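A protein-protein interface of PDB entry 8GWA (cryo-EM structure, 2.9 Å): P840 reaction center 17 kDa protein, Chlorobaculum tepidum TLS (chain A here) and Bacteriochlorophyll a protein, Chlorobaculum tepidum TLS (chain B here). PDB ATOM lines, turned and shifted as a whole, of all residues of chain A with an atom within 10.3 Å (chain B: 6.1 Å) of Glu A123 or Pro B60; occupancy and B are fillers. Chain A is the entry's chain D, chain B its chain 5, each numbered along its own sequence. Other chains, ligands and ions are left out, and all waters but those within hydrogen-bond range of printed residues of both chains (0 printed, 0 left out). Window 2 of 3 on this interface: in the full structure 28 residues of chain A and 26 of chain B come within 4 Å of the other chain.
Glu A123 touches just one residue of chain B: Pro B60. Printed residues of chain B within 4 Å of Gly A124: Pro B60 (2.7 Å) and Ala B61 (3.2 Å). Printed residues of chain B within 4 Å of Lys A125: Asp B246 (3.2 Å). Leu A127 touches none of the printed residues of chain B. Leu B58 touches none of the printed residues of chain A. No residue of chain A comes within 4 Å of Asp B59. Of chain A, only His A122 (3.5 Å), Glu A123 (3.1 Å) and Gly A124 (2.7 Å) come within 4 Å of Pro B60. Of chain A, only Gly A124 (3.2 Å) comes within 4 Å of Ala B61. No residue of chain A comes within 4 Å of Gly B63. The nearest residue of chain B that does not touch Glu A123 is Ala B61 (4.3 Å).
Asp B246 touches Phe A120. CB of Pro B60 touches NE2 of His A122, 3.5 Å away. His A122 touches Asp B246 (CD2 to O, 3.0 Å). Leu B248 touches His A122 (O to CD2, 3.95 Å). Pro B60 touches Glu A123. Gly A124 touches Ala B61. Asp B246 touches Ile A135.
Hydrophobic or aromatic side chains of chain B that line the printed part of chain A: Pro B60. Printed residues of chain A that touch a printed residue of chain B: Phe A120, His A122, Glu A123, Gly A124, Lys A125 and Ile A135. Hydrophobic or aromatic side chains of chain A that line the printed part of chain B: Phe A120, His A122 and Ile A135. Along chain A the printed residues that touch a printed residue of chain B span positions 120 to 135. Among the printed residues, Asp or Glu carboxylates within 4 Å of a Lys or Arg side-chain nitrogen of the other chain: Lys A125 with Asp B246 (3.5 Å).
The backbone NH (N) of Gly A124 lies within hydrogen-bond range of the backbone carbonyl oxygen (O) of Pro B60. OD1 of Asp B246 lies within salt-bridge range of NZ of Lys A125.
O of Phe A120 sits at hydrogen-bond distance from N of Cys A128 (2.9 Å).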
ATOM      1  N   PRO A  64      10.913   7.805  -3.698  1.00  0.00           N
ATOM      2  CA  PRO A  64      11.032   6.342  -3.798  1.00  0.00           C
ATOM      3  C   PRO A  64      11.722   5.697  -2.607  1.00  0.00           C
ATOM      4  O   PRO A  64      11.328   4.598  -2.197  1.00  0.00           O
ATOM      5  CB  PRO A  64      11.829   6.155  -5.093  1.00  0.00           C
ATOM      6  CG  PRO A  64      11.438   7.320  -5.926  1.00  0.00           C
ATOM      7  CD  PRO A  64      11.229   8.471  -4.976  1.00  0.00           C
ATOM      8  N   ILE A  67       9.388   5.645   0.313  1.00  0.00           N
ATOM      9  CA  ILE A  67       8.321   4.714  -0.046  1.00  0.00           C
ATOM     10  C   ILE A  67       8.767   3.276   0.190  1.00  0.00           C
ATOM     11  O   ILE A  67       8.024   2.460   0.751  1.00  0.00           O
ATOM     12  CB  ILE A  67       7.881   4.945  -1.505  1.00  0.00           C
ATOM     13  CG1 ILE A  67       6.907   6.121  -1.589  1.00  0.00           C
ATOM     14  CG2 ILE A  67       7.279   3.681  -2.096  1.00  0.00           C
ATOM     15  CD1 ILE A  67       6.763   6.697  -2.979  1.00  0.00           C
ATOM     16  N   ARG A  68       9.993   2.949  -0.228  1.00  0.00           N
ATOM     17  CA  ARG A  68      10.542   1.622   0.029  1.00  0.00           C
ATOM     18  C   ARG A  68      10.688   1.367   1.523  1.00  0.00           C
ATOM     19  O   ARG A  68      10.395   0.266   2.005  1.00  0.00           O
ATOM     20  CB  ARG A  68      11.886   1.472  -0.682  1.00  0.00           C
ATOM     21  CG  ARG A  68      12.695   0.261  -0.258  1.00  0.00           C
ATOM     22  CD  ARG A  68      14.162   0.622  -0.101  1.00  0.00           C
ATOM     23  NE  ARG A  68      14.398   1.506   1.035  1.00  0.00           N
ATOM     24  CZ  ARG A  68      14.812   1.102   2.227  1.00  0.00           C
ATOM     25  NH1 ARG A  68      15.045  -0.175   2.483  1.00  0.00           N
ATOM     26  NH2 ARG A  68      15.002   2.004   3.188  1.00  0.00           N
ATOM     27  N   LEU A  70       8.858   2.636   3.809  1.00  0.00           N
ATOM     28  CA  LEU A  70       7.494   2.386   4.265  1.00  0.00           C
ATOM     29  C   LEU A  70       7.092   0.940   4.018  1.00  0.00           C
ATOM     30  O   LEU A  70       6.713   0.220   4.949  1.00  0.00           O
ATOM     31  CB  LEU A  70       6.524   3.330   3.553  1.00  0.00           C
ATOM     32  CG  LEU A  70       5.024   3.137   3.804  1.00  0.00           C
ATOM     33  CD1 LEU A  70       4.715   2.886   5.278  1.00  0.00           C
ATOM     34  CD2 LEU A  70       4.212   4.299   3.259  1.00  0.00           C
ATOM     35  N   ILE A  71       7.171   0.494   2.759  1.00  0.00           N
ATOM     36  CA  ILE A  71       6.718  -0.853   2.411  1.00  0.00           C
ATOM     37  C   ILE A  71       7.646  -1.935   2.937  1.00  0.00           C
ATOM     38  O   ILE A  71       7.376  -3.123   2.723  1.00  0.00           O
ATOM     39  CB  ILE A  71       6.556  -1.008   0.886  1.00  0.00           C
ATOM     40  CG1 ILE A  71       7.895  -0.807   0.178  1.00  0.00           C
ATOM     41  CG2 ILE A  71       5.519  -0.025   0.364  1.00  0.00           C
ATOM     42  CD1 ILE A  71       7.780  -0.699  -1.329  1.00  0.00           C
ATOM     43  N   PHE A 120      -0.973   4.373   3.709  1.00  0.00           N
ATOM     44  CA  PHE A 120      -0.301   3.205   3.164  1.00  0.00           C
ATOM     45  C   PHE A 120      -0.039   3.404   1.676  1.00  0.00           C
ATOM     46  O   PHE A 120      -0.672   4.233   1.016  1.00  0.00           O
ATOM     47  CB  PHE A 120      -1.119   1.926   3.397  1.00  0.00           C
ATOM     48  CG  PHE A 120      -2.430   1.895   2.660  1.00  0.00           C
ATOM     49  CD1 PHE A 120      -3.532   2.582   3.144  1.00  0.00           C
ATOM     50  CD2 PHE A 120      -2.561   1.170   1.489  1.00  0.00           C
ATOM     51  CE1 PHE A 120      -4.736   2.550   2.467  1.00  0.00           C
ATOM     52  CE2 PHE A 120      -3.764   1.135   0.810  1.00  0.00           C
ATOM     53  CZ  PHE A 120      -4.851   1.827   1.299  1.00  0.00           C
ATOM     54  N   TYR A 121       0.906   2.627   1.152  1.00  0.00           N
ATOM     55  CA  TYR A 121       1.329   2.720  -0.241  1.00  0.00           C
ATOM     56  C   TYR A 121       1.071   1.388  -0.925  1.00  0.00           C
ATOM     57  O   TYR A 121       1.631   0.364  -0.521  1.00  0.00           O
ATOM     58  CB  TYR A 121       2.814   3.080  -0.345  1.00  0.00           C
ATOM     59  CG  TYR A 121       3.308   3.228  -1.766  1.00  0.00           C
ATOM     60  CD1 TYR A 121       3.007   4.358  -2.513  1.00  0.00           C
ATOM     61  CD2 TYR A 121       4.050   2.222  -2.371  1.00  0.00           C
ATOM     62  CE1 TYR A 121       3.454   4.493  -3.815  1.00  0.00           C
ATOM     63  CE2 TYR A 121       4.496   2.345  -3.673  1.00  0.00           C
ATOM     64  CZ  TYR A 121       4.196   3.483  -4.390  1.00  0.00           C
ATOM     65  OH  TYR A 121       4.636   3.616  -5.687  1.00  0.00           O
ATOM     66  N   HIS A 122       0.230   1.398  -1.960  1.00  0.00           N
ATOM     67  CA  HIS A 122       0.008   0.181  -2.740  1.00  0.00           C
ATOM     68  C   HIS A 122       1.094   0.002  -3.797  1.00  0.00           C
ATOM     69  O   HIS A 122       1.930  -0.901  -3.689  1.00  0.00           O
ATOM     70  CB  HIS A 122      -1.380   0.225  -3.386  1.00  0.00           C
ATOM     71  CG  HIS A 122      -1.662  -0.932  -4.293  1.00  0.00           C
ATOM     72  ND1 HIS A 122      -2.244  -0.781  -5.532  1.00  0.00           N
ATOM     73  CD2 HIS A 122      -1.435  -2.258  -4.144  1.00  0.00           C
ATOM     74  CE1 HIS A 122      -2.369  -1.963  -6.106  1.00  0.00           C
ATOM     75  NE2 HIS A 122      -1.886  -2.877  -5.283  1.00  0.00           N
ATOM     76  N   GLU A 123       1.110   0.903  -4.790  1.00  0.00           N
ATOM     77  CA  GLU A 123       2.050   0.990  -5.911  1.00  0.00           C
ATOM     78  C   GLU A 123       1.372   1.653  -7.103  1.00  0.00           C
ATOM     79  O   GLU A 123       1.792   2.731  -7.538  1.00  0.00           O
ATOM     80  CB  GLU A 123       2.609  -0.371  -6.341  1.00  0.00           C
ATOM     81  CG  GLU A 123       4.057  -0.300  -6.804  1.00  0.00           C
ATOM     82  CD  GLU A 123       4.687  -1.664  -6.985  1.00  0.00           C
ATOM     83  OE1 GLU A 123       4.465  -2.538  -6.124  1.00  0.00           O
ATOM     84  OE2 GLU A 123       5.404  -1.863  -7.988  1.00  0.00           O
ATOM     85  N   GLY A 124       0.334   1.009  -7.646  1.00  0.00           N
ATOM     86  CA  GLY A 124      -0.370   1.583  -8.784  1.00  0.00           C
ATOM     87  C   GLY A 124      -0.935   2.956  -8.483  1.00  0.00           C
ATOM     88  O   GLY A 124      -0.781   3.890  -9.274  1.00  0.00           O
ATOM     89  N   LYS A 125      -1.596   3.096  -7.342  1.00  0.00           N
ATOM     90  CA  LYS A 125      -1.871   4.397  -6.760  1.00  0.00           C
ATOM     91  C   LYS A 125      -0.801   4.692  -5.718  1.00  0.00           C
ATOM     92  O   LYS A 125      -0.238   3.778  -5.109  1.00  0.00           O
ATOM     93  CB  LYS A 125      -3.266   4.447  -6.135  1.00  0.00           C
ATOM     94  CG  LYS A 125      -3.576   3.300  -5.190  1.00  0.00           C
ATOM     95  CD  LYS A 125      -4.939   3.488  -4.546  1.00  0.00           C
ATOM     96  CE  LYS A 125      -6.050   3.393  -5.578  1.00  0.00           C
ATOM     97  NZ  LYS A 125      -7.398   3.511  -4.956  1.00  0.00           N
ATOM     98  N   GLY A 126      -0.519   5.974  -5.519  1.00  0.00           N
ATOM     99  CA  GLY A 126       0.600   6.349  -4.681  1.00  0.00           C
ATOM    100  C   GLY A 126       0.288   6.243  -3.205  1.00  0.00           C
ATOM    101  O   GLY A 126      -0.322   5.265  -2.763  1.00  0.00           O
ATOM    102  N   LEU A 127       0.708   7.233  -2.425  1.00  0.00           N
ATOM    103  CA  LEU A 127       0.395   7.247  -1.001  1.00  0.00           C
ATOM    104  C   LEU A 127      -1.103   7.465  -0.855  1.00  0.00           C
ATOM    105  O   LEU A 127      -1.606   8.575  -1.038  1.00  0.00           O
ATOM    106  CB  LEU A 127       1.191   8.331  -0.280  1.00  0.00           C
ATOM    107  CG  LEU A 127       2.629   8.021   0.147  1.00  0.00           C
ATOM    108  CD1 LEU A 127       2.648   6.902   1.176  1.00  0.00           C
ATOM    109  CD2 LEU A 127       3.530   7.689  -1.035  1.00  0.00           C
ATOM    110  N   CYS A 128      -1.825   6.399  -0.530  1.00  0.00           N
ATOM    111  CA  CYS A 128      -3.278   6.420  -0.478  1.00  0.00           C
ATOM    112  C   CYS A 128      -3.756   6.133   0.938  1.00  0.00           C
ATOM    113  O   CYS A 128      -3.205   5.271   1.629  1.00  0.00           O
ATOM    114  CB  CYS A 128      -3.873   5.400  -1.452  1.00  0.00           C
ATOM    115  SG  CYS A 128      -3.119   3.763  -1.375  1.00  0.00           S
ATOM    116  N   ILE A 135     -11.173   4.342  -0.359  1.00  0.00           N
ATOM    117  CA  ILE A 135      -9.718   4.440  -0.458  1.00  0.00           C
ATOM    118  C   ILE A 135      -9.411   5.730  -1.216  1.00  0.00           C
ATOM    119  O   ILE A 135      -9.520   5.791  -2.445  1.00  0.00           O
ATOM    120  CB  ILE A 135      -9.088   3.227  -1.148  1.00  0.00           C
ATOM    121  CG1 ILE A 135      -9.318   1.967  -0.311  1.00  0.00           C
ATOM    122  CG2 ILE A 135      -7.601   3.449  -1.365  1.00  0.00           C
ATOM    123  CD1 ILE A 135      -8.590   0.749  -0.823  1.00  0.00           C
ATOM    124  N   THR A 137      -6.621   8.739  -2.296  1.00  0.00           N
ATOM    125  CA  THR A 137      -5.204   8.883  -2.595  1.00  0.00           C
ATOM    126  C   THR A 137      -4.771  10.312  -2.305  1.00  0.00           C
ATOM    127  O   THR A 137      -5.526  11.257  -2.544  1.00  0.00           O
ATOM    128  CB  THR A 137      -4.906   8.537  -4.056  1.00  0.00           C
ATOM    129  OG1 THR A 137      -5.585   9.461  -4.915  1.00  0.00           O
ATOM    130  CG2 THR A 137      -5.369   7.128  -4.377  1.00  0.00           C
ATOM    131  N   ASP A 139      -2.417  11.812  -3.942  1.00  0.00           N
ATOM    132  CA  ASP A 139      -2.405  12.363  -5.292  1.00  0.00           C
ATOM    133  C   ASP A 139      -3.827  12.690  -5.721  1.00  0.00           C
ATOM    134  O   ASP A 139      -4.647  11.784  -5.905  1.00  0.00           O
ATOM    135  CB  ASP A 139      -1.760  11.386  -6.276  1.00  0.00           C
ATOM    136  CG  ASP A 139      -1.610  11.976  -7.664  1.00  0.00           C
ATOM    137  OD1 ASP A 139      -0.714  12.824  -7.859  1.00  0.00           O
ATOM    138  OD2 ASP A 139      -2.390  11.593  -8.561  1.00  0.00           O
ATOM    139  N   PRO B  57      -0.220 -10.432  -5.387  1.00  0.00           N
ATOM    140  CA  PRO B  57      -0.086  -9.451  -6.471  1.00  0.00           C
ATOM    141  C   PRO B  57       0.787  -9.985  -7.598  1.00  0.00           C
ATOM    142  O   PRO B  57       1.789 -10.665  -7.366  1.00  0.00           O
ATOM    143  CB  PRO B  57       0.561  -8.243  -5.781  1.00  0.00           C
ATOM    144  CG  PRO B  57       0.318  -8.450  -4.317  1.00  0.00           C
ATOM    145  CD  PRO B  57       0.316  -9.928  -4.113  1.00  0.00           C
ATOM    146  N   LEU B  58       0.392  -9.670  -8.831  1.00  0.00           N
ATOM    147  CA  LEU B  58       1.207  -9.982 -10.000  1.00  0.00           C
ATOM    148  C   LEU B  58       2.090  -8.795 -10.369  1.00  0.00           C
ATOM    149  O   LEU B  58       3.319  -8.908 -10.401  1.00  0.00           O
ATOM    150  CB  LEU B  58       0.311 -10.381 -11.178  1.00  0.00           C
ATOM    151  CG  LEU B  58      -0.088 -11.854 -11.254  1.00  0.00           C
ATOM    152  CD1 LEU B  58      -0.876 -12.120 -12.522  1.00  0.00           C
ATOM    153  CD2 LEU B  58       1.136 -12.749 -11.182  1.00  0.00           C
ATOM    154  N   ASP B  59       1.469  -7.652 -10.653  1.00  0.00           N
ATOM    155  CA  ASP B  59       2.171  -6.374 -10.739  1.00  0.00           C
ATOM    156  C   ASP B  59       1.251  -5.305 -10.161  1.00  0.00           C
ATOM    157  O   ASP B  59       0.305  -4.857 -10.828  1.00  0.00           O
ATOM    158  CB  ASP B  59       2.603  -6.042 -12.167  1.00  0.00           C
ATOM    159  CG  ASP B  59       1.452  -6.047 -13.152  1.00  0.00           C
ATOM    160  OD1 ASP B  59       0.441  -6.720 -12.878  1.00  0.00           O
ATOM    161  OD2 ASP B  59       1.555  -5.373 -14.199  1.00  0.00           O
ATOM    162  N   PRO B  60       1.488  -4.879  -8.917  1.00  0.00           N
ATOM    163  CA  PRO B  60       0.645  -3.832  -8.320  1.00  0.00           C
ATOM    164  C   PRO B  60       0.777  -2.480  -8.998  1.00  0.00           C
ATOM    165  O   PRO B  60       0.094  -1.536  -8.585  1.00  0.00           O
ATOM    166  CB  PRO B  60       1.116  -3.769  -6.858  1.00  0.00           C
ATOM    167  CG  PRO B  60       2.294  -4.656  -6.741  1.00  0.00           C
ATOM    168  CD  PRO B  60       2.578  -5.327  -8.035  1.00  0.00           C
ATOM    169  N   ALA B  61       1.637  -2.353 -10.012  1.00  0.00           N
ATOM    170  CA  ALA B  61       1.698  -1.119 -10.785  1.00  0.00           C
ATOM    171  C   ALA B  61       0.376  -0.831 -11.484  1.00  0.00           C
ATOM    172  O   ALA B  61       0.015   0.336 -11.668  1.00  0.00           O
ATOM    173  CB  ALA B  61       2.835  -1.192 -11.804  1.00  0.00           C
ATOM    174  N   LYS B  62      -0.353  -1.874 -11.889  1.00  0.00           N
ATOM    175  CA  LYS B  62      -1.671  -1.697 -12.478  1.00  0.00           C
ATOM    176  C   LYS B  62      -2.733  -2.626 -11.901  1.00  0.00           C
ATOM    177  O   LYS B  62      -3.826  -2.711 -12.470  1.00  0.00           O
ATOM    178  CB  LYS B  62      -1.608  -1.864 -14.005  1.00  0.00           C
ATOM    179  CG  LYS B  62      -1.190  -3.238 -14.485  1.00  0.00           C
ATOM    180  CD  LYS B  62      -1.193  -3.285 -16.004  1.00  0.00           C
ATOM    181  CE  LYS B  62      -0.038  -2.478 -16.578  1.00  0.00           C
ATOM    182  NZ  LYS B  62       0.054  -2.597 -18.060  1.00  0.00           N
ATOM    183  N   GLY B  63      -2.451  -3.319 -10.802  1.00  0.00           N
ATOM    184  CA  GLY B  63      -3.485  -3.949 -10.009  1.00  0.00           C
ATOM    185  C   GLY B  63      -3.701  -5.437 -10.187  1.00  0.00           C
ATOM    186  O   GLY B  63      -4.554  -5.996  -9.489  1.00  0.00           O
ATOM    187  N   PHE B  64      -2.981  -6.093 -11.096  1.00  0.00           N
ATOM    188  CA  PHE B  64      -3.152  -7.534 -11.264  1.00  0.00           C
ATOM    189  C   PHE B  64      -2.824  -8.273  -9.975  1.00  0.00           C
ATOM    190  O   PHE B  64      -1.779  -8.044  -9.358  1.00  0.00           O
ATOM    191  CB  PHE B  64      -2.265  -8.060 -12.395  1.00  0.00           C
ATOM    192  CG  PHE B  64      -2.780  -7.764 -13.774  1.00  0.00           C
ATOM    193  CD1 PHE B  64      -4.123  -7.534 -13.995  1.00  0.00           C
ATOM    194  CD2 PHE B  64      -1.914  -7.732 -14.855  1.00  0.00           C
ATOM    195  CE1 PHE B  64      -4.597  -7.267 -15.265  1.00  0.00           C
ATOM    196  CE2 PHE B  64      -2.381  -7.465 -16.128  1.00  0.00           C
ATOM    197  CZ  PHE B  64      -3.726  -7.233 -16.332  1.00  0.00           C
ATOM    198  N   ASP B 246      -5.919  -2.724  -3.533  1.00  0.00           N
ATOM    199  CA  ASP B 246      -5.025  -1.644  -3.128  1.00  0.00           C
ATOM    200  C   ASP B 246      -4.294  -1.979  -1.835  1.00  0.00           C
ATOM    201  O   ASP B 246      -3.107  -1.674  -1.687  1.00  0.00           O
ATOM    202  CB  ASP B 246      -5.814  -0.343  -2.976  1.00  0.00           C
ATOM    203  CG  ASP B 246      -6.760  -0.098  -4.133  1.00  0.00           C
ATOM    204  OD1 ASP B 246      -6.277   0.216  -5.241  1.00  0.00           O
ATOM    205  OD2 ASP B 246      -7.988  -0.216  -3.935  1.00  0.00           O
ATOM    206  N   LEU B 248      -3.577  -4.987  -0.584  1.00  0.00           N
ATOM    207  CA  LEU B 248      -2.941  -6.298  -0.610  1.00  0.00           C
ATOM    208  C   LEU B 248      -1.446  -6.103  -0.824  1.00  0.00           C
ATOM    209  O   LEU B 248      -1.042  -5.363  -1.728  1.00  0.00           O
ATOM    210  CB  LEU B 248      -3.514  -7.171  -1.729  1.00  0.00           C
ATOM    211  CG  LEU B 248      -2.939  -8.588  -1.833  1.00  0.00           C
ATOM    212  CD1 LEU B 248      -3.324  -9.423  -0.624  1.00  0.00           C
ATOM    213  CD2 LEU B 248      -3.342  -9.275  -3.126  1.00  0.00           C
